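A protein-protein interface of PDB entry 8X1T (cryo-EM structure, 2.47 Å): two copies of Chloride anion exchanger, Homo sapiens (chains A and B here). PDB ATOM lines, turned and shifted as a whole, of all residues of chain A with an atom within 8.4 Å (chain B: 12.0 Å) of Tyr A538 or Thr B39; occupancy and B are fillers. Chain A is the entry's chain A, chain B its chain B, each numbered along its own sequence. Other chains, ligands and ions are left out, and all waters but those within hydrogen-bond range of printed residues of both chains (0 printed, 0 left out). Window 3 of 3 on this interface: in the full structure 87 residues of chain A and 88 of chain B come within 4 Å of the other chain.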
ATOM      1  N   ASN A 524     -11.507   3.399   3.052  1.00  0.00           N
ATOM      2  CA  ASN A 524     -12.891   3.020   2.917  1.00  0.00           C
ATOM      3  C   ASN A 524     -13.683   3.650   4.044  1.00  0.00           C
ATOM      4  O   ASN A 524     -13.157   3.844   5.132  1.00  0.00           O
ATOM      5  CB  ASN A 524     -13.036   1.501   2.944  1.00  0.00           C
ATOM      6  CG  ASN A 524     -14.255   1.021   2.195  1.00  0.00           C
ATOM      7  OD1 ASN A 524     -14.711   1.665   1.256  1.00  0.00           O
ATOM      8  ND2 ASN A 524     -14.780  -0.126   2.595  1.00  0.00           N
ATOM      9  N   ILE A 525     -14.943   3.981   3.790  1.00  0.00           N
ATOM     10  CA  ILE A 525     -15.797   4.524   4.842  1.00  0.00           C
ATOM     11  C   ILE A 525     -17.217   3.958   4.770  1.00  0.00           C
ATOM     12  O   ILE A 525     -17.991   4.342   3.898  1.00  0.00           O
ATOM     13  CB  ILE A 525     -15.809   6.070   4.802  1.00  0.00           C
ATOM     14  CG1 ILE A 525     -16.846   6.624   5.781  1.00  0.00           C
ATOM     15  CG2 ILE A 525     -16.059   6.572   3.387  1.00  0.00           C
ATOM     16  CD1 ILE A 525     -16.771   8.122   5.960  1.00  0.00           C
ATOM     17  N   GLY A 526     -17.560   3.039   5.670  1.00  0.00           N
ATOM     18  CA  GLY A 526     -18.887   2.432   5.677  1.00  0.00           C
ATOM     19  C   GLY A 526     -18.907   1.002   5.189  1.00  0.00           C
ATOM     20  O   GLY A 526     -19.953   0.528   4.759  1.00  0.00           O
ATOM     21  N   ASN A 533     -11.087  10.803   1.623  1.00  0.00           N
ATOM     22  CA  ASN A 533      -9.812  11.220   2.192  1.00  0.00           C
ATOM     23  C   ASN A 533      -9.594  10.605   3.566  1.00  0.00           C
ATOM     24  O   ASN A 533     -10.452  10.693   4.444  1.00  0.00           O
ATOM     25  CB  ASN A 533      -9.761  12.742   2.289  1.00  0.00           C
ATOM     26  CG  ASN A 533      -8.354  13.276   2.300  1.00  0.00           C
ATOM     27  OD1 ASN A 533      -7.444  12.650   2.833  1.00  0.00           O
ATOM     28  ND2 ASN A 533      -8.165  14.446   1.714  1.00  0.00           N
ATOM     29  N   LYS A 534      -8.422   9.996   3.750  1.00  0.00           N
ATOM     30  CA  LYS A 534      -8.104   9.294   4.988  1.00  0.00           C
ATOM     31  C   LYS A 534      -8.104  10.217   6.198  1.00  0.00           C
ATOM     32  O   LYS A 534      -8.246   9.742   7.329  1.00  0.00           O
ATOM     33  CB  LYS A 534      -6.744   8.617   4.839  1.00  0.00           C
ATOM     34  CG  LYS A 534      -6.341   7.689   5.949  1.00  0.00           C
ATOM     35  CD  LYS A 534      -4.856   7.405   5.861  1.00  0.00           C
ATOM     36  CE  LYS A 534      -4.342   6.727   7.113  1.00  0.00           C
ATOM     37  NZ  LYS A 534      -2.891   6.420   7.004  1.00  0.00           N
ATOM     38  N   LYS A 535      -7.956  11.521   5.985  1.00  0.00           N
ATOM     39  CA  LYS A 535      -7.855  12.491   7.062  1.00  0.00           C
ATOM     40  C   LYS A 535      -9.148  13.247   7.316  1.00  0.00           C
ATOM     41  O   LYS A 535      -9.141  14.210   8.086  1.00  0.00           O
ATOM     42  CB  LYS A 535      -6.743  13.493   6.751  1.00  0.00           C
ATOM     43  CG  LYS A 535      -5.377  12.871   6.591  1.00  0.00           C
ATOM     44  CD  LYS A 535      -4.288  13.912   6.730  1.00  0.00           C
ATOM     45  CE  LYS A 535      -4.482  15.039   5.738  1.00  0.00           C
ATOM     46  NZ  LYS A 535      -3.258  15.872   5.619  1.00  0.00           N
ATOM     47  N   ASP A 536     -10.255  12.840   6.701  1.00  0.00           N
ATOM     48  CA  ASP A 536     -11.462  13.651   6.703  1.00  0.00           C
ATOM     49  C   ASP A 536     -12.562  13.131   7.615  1.00  0.00           C
ATOM     50  O   ASP A 536     -13.320  13.937   8.156  1.00  0.00           O
ATOM     51  CB  ASP A 536     -12.016  13.773   5.285  1.00  0.00           C
ATOM     52  CG  ASP A 536     -11.425  14.939   4.532  1.00  0.00           C
ATOM     53  OD1 ASP A 536     -10.482  15.565   5.049  1.00  0.00           O
ATOM     54  OD2 ASP A 536     -11.905  15.237   3.420  1.00  0.00           O
ATOM     55  N   TYR A 537     -12.680  11.823   7.810  1.00  0.00           N
ATOM     56  CA  TYR A 537     -13.785  11.271   8.573  1.00  0.00           C
ATOM     57  C   TYR A 537     -13.257  10.384   9.690  1.00  0.00           C
ATOM     58  O   TYR A 537     -12.079  10.027   9.727  1.00  0.00           O
ATOM     59  CB  TYR A 537     -14.749  10.468   7.687  1.00  0.00           C
ATOM     60  CG  TYR A 537     -15.309  11.247   6.519  1.00  0.00           C
ATOM     61  CD1 TYR A 537     -16.584  11.783   6.568  1.00  0.00           C
ATOM     62  CD2 TYR A 537     -14.566  11.438   5.366  1.00  0.00           C
ATOM     63  CE1 TYR A 537     -17.096  12.496   5.509  1.00  0.00           C
ATOM     64  CE2 TYR A 537     -15.068  12.150   4.306  1.00  0.00           C
ATOM     65  CZ  TYR A 537     -16.332  12.673   4.382  1.00  0.00           C
ATOM     66  OH  TYR A 537     -16.836  13.383   3.319  1.00  0.00           O
ATOM     67  N   TYR A 538     -14.151  10.040  10.610  1.00  0.00           N
ATOM     68  CA  TYR A 538     -13.842   9.093  11.666  1.00  0.00           C
ATOM     69  C   TYR A 538     -14.260   7.686  11.254  1.00  0.00           C
ATOM     70  O   TYR A 538     -15.088   7.492  10.360  1.00  0.00           O
ATOM     71  CB  TYR A 538     -14.556   9.472  12.965  1.00  0.00           C
ATOM     72  CG  TYR A 538     -14.023  10.708  13.648  1.00  0.00           C
ATOM     73  CD1 TYR A 538     -12.727  10.751  14.140  1.00  0.00           C
ATOM     74  CD2 TYR A 538     -14.825  11.827  13.817  1.00  0.00           C
ATOM     75  CE1 TYR A 538     -12.242  11.876  14.770  1.00  0.00           C
ATOM     76  CE2 TYR A 538     -14.346  12.956  14.444  1.00  0.00           C
ATOM     77  CZ  TYR A 538     -13.056  12.974  14.920  1.00  0.00           C
ATOM     78  OH  TYR A 538     -12.578  14.101  15.548  1.00  0.00           O
ATOM     79  N   ASP A 539     -13.670   6.696  11.923  1.00  0.00           N
ATOM     80  CA  ASP A 539     -14.047   5.293  11.762  1.00  0.00           C
ATOM     81  C   ASP A 539     -13.802   4.787  10.343  1.00  0.00           C
ATOM     82  O   ASP A 539     -14.532   3.928   9.846  1.00  0.00           O
ATOM     83  CB  ASP A 539     -15.508   5.064  12.160  1.00  0.00           C
ATOM     84  CG  ASP A 539     -15.683   4.869  13.649  1.00  0.00           C
ATOM     85  OD1 ASP A 539     -14.753   5.212  14.411  1.00  0.00           O
ATOM     86  OD2 ASP A 539     -16.752   4.377  14.062  1.00  0.00           O
ATOM     87  N   MET A 540     -12.776   5.306   9.679  1.00  0.00           N
ATOM     88  CA  MET A 540     -12.399   4.812   8.366  1.00  0.00           C
ATOM     89  C   MET A 540     -11.563   3.544   8.502  1.00  0.00           C
ATOM     90  O   MET A 540     -11.194   3.132   9.604  1.00  0.00           O
ATOM     91  CB  MET A 540     -11.636   5.878   7.588  1.00  0.00           C
ATOM     92  CG  MET A 540     -12.380   7.191   7.498  1.00  0.00           C
ATOM     93  SD  MET A 540     -11.479   8.442   6.584  1.00  0.00           S
ATOM     94  CE  MET A 540     -12.271   8.289   5.001  1.00  0.00           C
ATOM     95  N   TYR A 541     -11.269   2.919   7.365  1.00  0.00           N
ATOM     96  CA  TYR A 541     -10.653   1.595   7.361  1.00  0.00           C
ATOM     97  C   TYR A 541      -9.677   1.489   6.200  1.00  0.00           C
ATOM     98  O   TYR A 541     -10.054   1.701   5.045  1.00  0.00           O
ATOM     99  CB  TYR A 541     -11.718   0.502   7.276  1.00  0.00           C
ATOM    100  CG  TYR A 541     -11.182  -0.861   6.924  1.00  0.00           C
ATOM    101  CD1 TYR A 541     -11.370  -1.395   5.660  1.00  0.00           C
ATOM    102  CD2 TYR A 541     -10.497  -1.621   7.860  1.00  0.00           C
ATOM    103  CE1 TYR A 541     -10.886  -2.643   5.333  1.00  0.00           C
ATOM    104  CE2 TYR A 541     -10.008  -2.871   7.542  1.00  0.00           C
ATOM    105  CZ  TYR A 541     -10.207  -3.376   6.277  1.00  0.00           C
ATOM    106  OH  TYR A 541      -9.723  -4.621   5.953  1.00  0.00           O
ATOM    107  N   TYR B  27     -26.789   7.889  -1.521  1.00  0.00           N
ATOM    108  CA  TYR B  27     -26.148   8.964  -0.778  1.00  0.00           C
ATOM    109  C   TYR B  27     -25.992  10.190  -1.656  1.00  0.00           C
ATOM    110  O   TYR B  27     -25.356  10.127  -2.714  1.00  0.00           O
ATOM    111  CB  TYR B  27     -24.780   8.525  -0.255  1.00  0.00           C
ATOM    112  CG  TYR B  27     -24.817   7.860   1.096  1.00  0.00           C
ATOM    113  CD1 TYR B  27     -25.516   8.426   2.146  1.00  0.00           C
ATOM    114  CD2 TYR B  27     -24.150   6.669   1.320  1.00  0.00           C
ATOM    115  CE1 TYR B  27     -25.553   7.824   3.376  1.00  0.00           C
ATOM    116  CE2 TYR B  27     -24.181   6.061   2.548  1.00  0.00           C
ATOM    117  CZ  TYR B  27     -24.884   6.644   3.574  1.00  0.00           C
ATOM    118  OH  TYR B  27     -24.922   6.043   4.809  1.00  0.00           O
ATOM    119  N   PHE B  32     -24.256  12.027   2.879  1.00  0.00           N
ATOM    120  CA  PHE B  32     -23.102  11.260   3.304  1.00  0.00           C
ATOM    121  C   PHE B  32     -22.395  11.995   4.429  1.00  0.00           C
ATOM    122  O   PHE B  32     -21.987  11.388   5.407  1.00  0.00           O
ATOM    123  CB  PHE B  32     -22.149  11.011   2.140  1.00  0.00           C
ATOM    124  CG  PHE B  32     -20.965  10.170   2.507  1.00  0.00           C
ATOM    125  CD1 PHE B  32     -21.033   8.791   2.430  1.00  0.00           C
ATOM    126  CD2 PHE B  32     -19.790  10.757   2.941  1.00  0.00           C
ATOM    127  CE1 PHE B  32     -19.949   8.015   2.772  1.00  0.00           C
ATOM    128  CE2 PHE B  32     -18.702   9.985   3.285  1.00  0.00           C
ATOM    129  CZ  PHE B  32     -18.783   8.612   3.199  1.00  0.00           C
ATOM    130  N   GLU B  33     -22.262  13.303   4.290  1.00  0.00           N
ATOM    131  CA  GLU B  33     -21.592  14.101   5.308  1.00  0.00           C
ATOM    132  C   GLU B  33     -22.383  14.205   6.604  1.00  0.00           C
ATOM    133  O   GLU B  33     -21.805  14.394   7.667  1.00  0.00           O
ATOM    134  CB  GLU B  33     -21.299  15.495   4.760  1.00  0.00           C
ATOM    135  CG  GLU B  33     -20.326  15.483   3.592  1.00  0.00           C
ATOM    136  CD  GLU B  33     -20.316  16.786   2.822  1.00  0.00           C
ATOM    137  OE1 GLU B  33     -19.394  16.984   2.002  1.00  0.00           O
ATOM    138  OE2 GLU B  33     -21.229  17.613   3.034  1.00  0.00           O
ATOM    139  N   GLU B  34     -23.699  14.088   6.523  1.00  0.00           N
ATOM    140  CA  GLU B  34     -24.533  14.165   7.709  1.00  0.00           C
ATOM    141  C   GLU B  34     -24.605  12.829   8.434  1.00  0.00           C
ATOM    142  O   GLU B  34     -25.080  12.762   9.563  1.00  0.00           O
ATOM    143  CB  GLU B  34     -25.934  14.637   7.339  1.00  0.00           C
ATOM    144  CG  GLU B  34     -26.826  13.555   6.761  1.00  0.00           C
ATOM    145  CD  GLU B  34     -28.041  14.122   6.057  1.00  0.00           C
ATOM    146  OE1 GLU B  34     -28.986  13.351   5.787  1.00  0.00           O
ATOM    147  OE2 GLU B  34     -28.048  15.339   5.774  1.00  0.00           O
ATOM    148  N   ASN B  35     -24.140  11.766   7.792  1.00  0.00           N
ATOM    149  CA  ASN B  35     -24.163  10.447   8.407  1.00  0.00           C
ATOM    150  C   ASN B  35     -22.766   9.994   8.769  1.00  0.00           C
ATOM    151  O   ASN B  35     -22.588   8.939   9.362  1.00  0.00           O
ATOM    152  CB  ASN B  35     -24.811   9.442   7.465  1.00  0.00           C
ATOM    153  CG  ASN B  35     -26.225   9.831   7.090  1.00  0.00           C
ATOM    154  OD1 ASN B  35     -26.954  10.406   7.896  1.00  0.00           O
ATOM    155  ND2 ASN B  35     -26.622   9.520   5.864  1.00  0.00           N
ATOM    156  N   HIS B  36     -21.772  10.789   8.409  1.00  0.00           N
ATOM    157  CA  HIS B  36     -20.402  10.438   8.708  1.00  0.00           C
ATOM    158  C   HIS B  36     -19.715  11.621   9.341  1.00  0.00           C
ATOM    159  O   HIS B  36     -19.654  12.695   8.751  1.00  0.00           O
ATOM    160  CB  HIS B  36     -19.679   9.990   7.438  1.00  0.00           C
ATOM    161  CG  HIS B  36     -20.309   8.800   6.787  1.00  0.00           C
ATOM    162  ND1 HIS B  36     -21.350   8.907   5.892  1.00  0.00           N
ATOM    163  CD2 HIS B  36     -20.066   7.476   6.925  1.00  0.00           C
ATOM    164  CE1 HIS B  36     -21.712   7.701   5.495  1.00  0.00           C
ATOM    165  NE2 HIS B  36     -20.947   6.815   6.106  1.00  0.00           N
ATOM    166  N   LYS B  37     -19.237  11.435  10.566  1.00  0.00           N
ATOM    167  CA  LYS B  37     -18.564  12.511  11.282  1.00  0.00           C
ATOM    168  C   LYS B  37     -17.306  12.926  10.557  1.00  0.00           C
ATOM    169  O   LYS B  37     -16.365  12.145  10.439  1.00  0.00           O
ATOM    170  CB  LYS B  37     -18.220  12.067  12.700  1.00  0.00           C
ATOM    171  N   LYS B  38     -17.289  14.157  10.074  1.00  0.00           N
ATOM    172  CA  LYS B  38     -16.130  14.636   9.355  1.00  0.00           C
ATOM    173  C   LYS B  38     -15.142  15.271  10.306  1.00  0.00           C
ATOM    174  O   LYS B  38     -15.449  16.267  10.945  1.00  0.00           O
ATOM    175  CB  LYS B  38     -16.544  15.637   8.283  1.00  0.00           C
ATOM    176  CG  LYS B  38     -15.583  15.697   7.109  1.00  0.00           C
ATOM    177  CD  LYS B  38     -16.205  16.408   5.922  1.00  0.00           C
ATOM    178  CE  LYS B  38     -15.265  16.396   4.728  1.00  0.00           C
ATOM    179  NZ  LYS B  38     -15.856  17.123   3.571  1.00  0.00           N
ATOM    180  N   THR B  39     -13.957  14.694  10.402  1.00  0.00           N
ATOM    181  CA  THR B  39     -12.927  15.260  11.246  1.00  0.00           C
ATOM    182  C   THR B  39     -12.817  16.737  10.956  1.00  0.00           C
ATOM    183  O   THR B  39     -12.655  17.139   9.805  1.00  0.00           O
ATOM    184  CB  THR B  39     -11.564  14.605  10.981  1.00  0.00           C
ATOM    185  OG1 THR B  39     -11.623  13.216  11.327  1.00  0.00           O
ATOM    186  CG2 THR B  39     -10.484  15.281  11.804  1.00  0.00           C
ATOM    187  N   GLY B  40     -12.914  17.553  11.992  1.00  0.00           N
ATOM    188  CA  GLY B  40     -12.825  18.983  11.809  1.00  0.00           C
ATOM    189  C   GLY B  40     -11.369  19.346  11.700  1.00  0.00           C
ATOM    190  O   GLY B  40     -10.615  19.181  12.656  1.00  0.00           O
ATOM    191  N   ARG B  41     -10.960  19.830  10.537  1.00  0.00           N
ATOM    192  CA  ARG B  41      -9.543  20.107  10.349  1.00  0.00           C
ATOM    193  C   ARG B  41      -9.354  21.593  10.092  1.00  0.00           C
ATOM    194  O   ARG B  41      -9.970  22.150   9.178  1.00  0.00           O
ATOM    195  CB  ARG B  41      -8.957  19.299   9.185  1.00  0.00           C
ATOM    196  CG  ARG B  41      -9.519  17.903   9.026  1.00  0.00           C
ATOM    197  CD  ARG B  41      -9.536  17.488   7.566  1.00  0.00           C
ATOM    198  NE  ARG B  41      -8.216  17.596   6.948  1.00  0.00           N
ATOM    199  CZ  ARG B  41      -7.996  17.514   5.640  1.00  0.00           C
ATOM    200  NH1 ARG B  41      -9.008  17.320   4.806  1.00  0.00           N
ATOM    201  NH2 ARG B  41      -6.765  17.625   5.162  1.00  0.00           N
ATOM    202  N   HIS B  42      -8.501  22.222  10.889  1.00  0.00           N
ATOM    203  CA  HIS B  42      -8.221  23.639  10.708  1.00  0.00           C
ATOM    204  C   HIS B  42      -7.206  23.830   9.602  1.00  0.00           C
ATOM    205  O   HIS B  42      -6.092  23.313   9.682  1.00  0.00           O
ATOM    206  CB  HIS B  42      -7.687  24.237  12.004  1.00  0.00           C
ATOM    207  CG  HIS B  42      -6.968  25.535  11.816  1.00  0.00           C
ATOM    208  ND1 HIS B  42      -5.601  25.611  11.651  1.00  0.00           N
ATOM    209  CD2 HIS B  42      -7.424  26.808  11.762  1.00  0.00           C
ATOM    210  CE1 HIS B  42      -5.246  26.875  11.509  1.00  0.00           C
ATOM    211  NE2 HIS B  42      -6.334  27.622  11.570  1.00  0.00           N
ATOM    212  N   HIS B  43      -7.583  24.565   8.563  1.00  0.00           N
ATOM    213  CA  HIS B  43      -6.650  24.845   7.483  1.00  0.00           C
ATOM    214  C   HIS B  43      -5.563  25.794   7.950  1.00  0.00           C
ATOM    215  O   HIS B  43      -5.818  26.684   8.760  1.00  0.00           O
ATOM    216  CB  HIS B  43      -7.381  25.453   6.290  1.00  0.00           C
ATOM    217  CG  HIS B  43      -6.543  26.408   5.496  1.00  0.00           C
ATOM    218  ND1 HIS B  43      -5.689  25.997   4.496  1.00  0.00           N
ATOM    219  CD2 HIS B  43      -6.423  27.755   5.563  1.00  0.00           C
ATOM    220  CE1 HIS B  43      -5.082  27.049   3.977  1.00  0.00           C
ATOM    221  NE2 HIS B  43      -5.509  28.128   4.608  1.00  0.00           N
ATOM    222  N   ASP B 699     -14.784  16.239  -1.976  1.00  0.00           N
ATOM    223  CA  ASP B 699     -15.269  17.256  -1.050  1.00  0.00           C
ATOM    224  C   ASP B 699     -14.564  18.591  -1.243  1.00  0.00           C
ATOM    225  O   ASP B 699     -15.162  19.645  -0.997  1.00  0.00           O
ATOM    226  CB  ASP B 699     -15.101  16.774   0.389  1.00  0.00           C
ATOM    227  CG  ASP B 699     -15.806  15.457   0.647  1.00  0.00           C
ATOM    228  OD1 ASP B 699     -15.310  14.671   1.482  1.00  0.00           O
ATOM    229  OD2 ASP B 699     -16.851  15.203   0.014  1.00  0.00           O
ATOM    230  N   ASP B 700     -13.306  18.571  -1.684  1.00  0.00           N
ATOM    231  CA  ASP B 700     -12.601  19.818  -1.953  1.00  0.00           C
ATOM    232  C   ASP B 700     -13.243  20.583  -3.101  1.00  0.00           C
ATOM    233  O   ASP B 700     -13.258  21.817  -3.091  1.00  0.00           O
ATOM    234  CB  ASP B 700     -11.132  19.533  -2.258  1.00  0.00           C
ATOM    235  CG  ASP B 700     -10.435  18.798  -1.133  1.00  0.00           C
ATOM    236  OD1 ASP B 700     -10.646  17.576  -0.994  1.00  0.00           O
ATOM    237  OD2 ASP B 700      -9.673  19.444  -0.382  1.00  0.00           O
ATOM    238  N   GLU B 703     -16.162  22.378  -1.756  1.00  0.00           N
ATOM    239  CA  GLU B 703     -15.703  23.462  -0.898  1.00  0.00           C
ATOM    240  C   GLU B 703     -15.331  24.703  -1.715  1.00  0.00           C
ATOM    241  O   GLU B 703     -15.761  25.812  -1.397  1.00  0.00           O
ATOM    242  CB  GLU B 703     -14.524  23.008  -0.044  1.00  0.00           C
ATOM    243  CG  GLU B 703     -13.876  24.133   0.741  1.00  0.00           C
ATOM    244  CD  GLU B 703     -14.885  24.965   1.509  1.00  0.00           C
ATOM    245  OE1 GLU B 703     -15.844  24.387   2.064  1.00  0.00           O
ATOM    246  OE2 GLU B 703     -14.719  26.203   1.561  1.00  0.00           O
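The side-chain carboxylate (OE1) of Glu B33 is in salt-bridge range of the side-chain amino group (NZ) of Lys B38 (3.9 Å). The side-chain carboxylate of Asp B699 is in salt-bridge range of the side-chain amino group of Lys B38, at 3.3 Å. The backbone NH (N) of Lys A535 sits close to the side-chain amide oxygen (OD1) of Asn A533, at 3.4 Å. The backbone carbonyl oxygen (O) of Phe B32 is in hydrogen-bond range of a ring nitrogen (ND1) of His B36 (2.6 Å). The backbone NH of Tyr A537 lies within hydrogen-bond range of the side-chain sulfur of Met A540 (3.8 Å).
No position is printed for both chains. Of the 16 pairs that touch across the chains among the printed residues, none has its exchanged pair printed and touching as well.
Phe B32 touches Ile A525. CD1 of Ile A525 touches CD2 of His B36, at 3.5 Å. Lys A535 touches Thr B39. Asp A536 touches Asp B699. Phe B32 touches Tyr A537. Tyr A537 touches His B36. Tyr A537 touches Lys B37. Lys B38 touches Tyr A537. Tyr A537 touches Thr B39. CE1 of Tyr A538 touches OG1 of Thr B39, at 3.7 Å.
The backbone NH (N) of Tyr A538 is in hydrogen-bond range of the backbone carbonyl oxygen (O) of Lys B37, at 3.1 Å. N of Thr B39 is in hydrogen-bond range of O of Asp A536 (2.5 Å). The guanidinium group (NE) of Arg B41 lies within salt-bridge range of the side-chain carboxylate (OD1) of Asp A536 (3.6 Å). The side-chain hydroxyl (OH) of Tyr A537 is in hydrogen-bond range of the side-chain carboxylate (OD1) of Asp B699, at 2.7 Å.
Ile A525 touches two residues of chain B. Tyr A537 touches six residues of chain B. Printed residues of chain B within 4 Å of Tyr A538: Lys B37 (3.1 Å) and Thr B39 (3.7 Å). No residue of chain B comes within 4 Å of Asp A539. No residue of chain B comes within 4 Å of Met A540. Printed residues of chain A within 4 Å of His B36: Ile A525 (3.5 Å) and Tyr A537 (3.7 Å). Thr B39 touches four residues of chain A. No residue of chain A comes within 4 Å of Gly B40. Printed residues of chain A within 4 Å of Asp B699: Asp A536 (3.96 Å) and Tyr A537 (2.7 Å). The nearest residue of chain B that does not touch Tyr A538 is Lys B38 (4.8 Å). The nearest printed residue of chain A that does not touch Lys B38 is Tyr A538 (4.8 Å).
Of the 16 printed residues of chain B, 7 touch a printed residue of chain A. Hydrophobic or aromatic side chains of chain B within 4 Å of the printed part of chain A: Phe B32 and His B36. Among the printed residues, Asp or Glu carboxylates within 4 Å of a Lys or Arg side-chain nitrogen of the other chain: Asp A536 with Arg B41 (2.3 Å).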
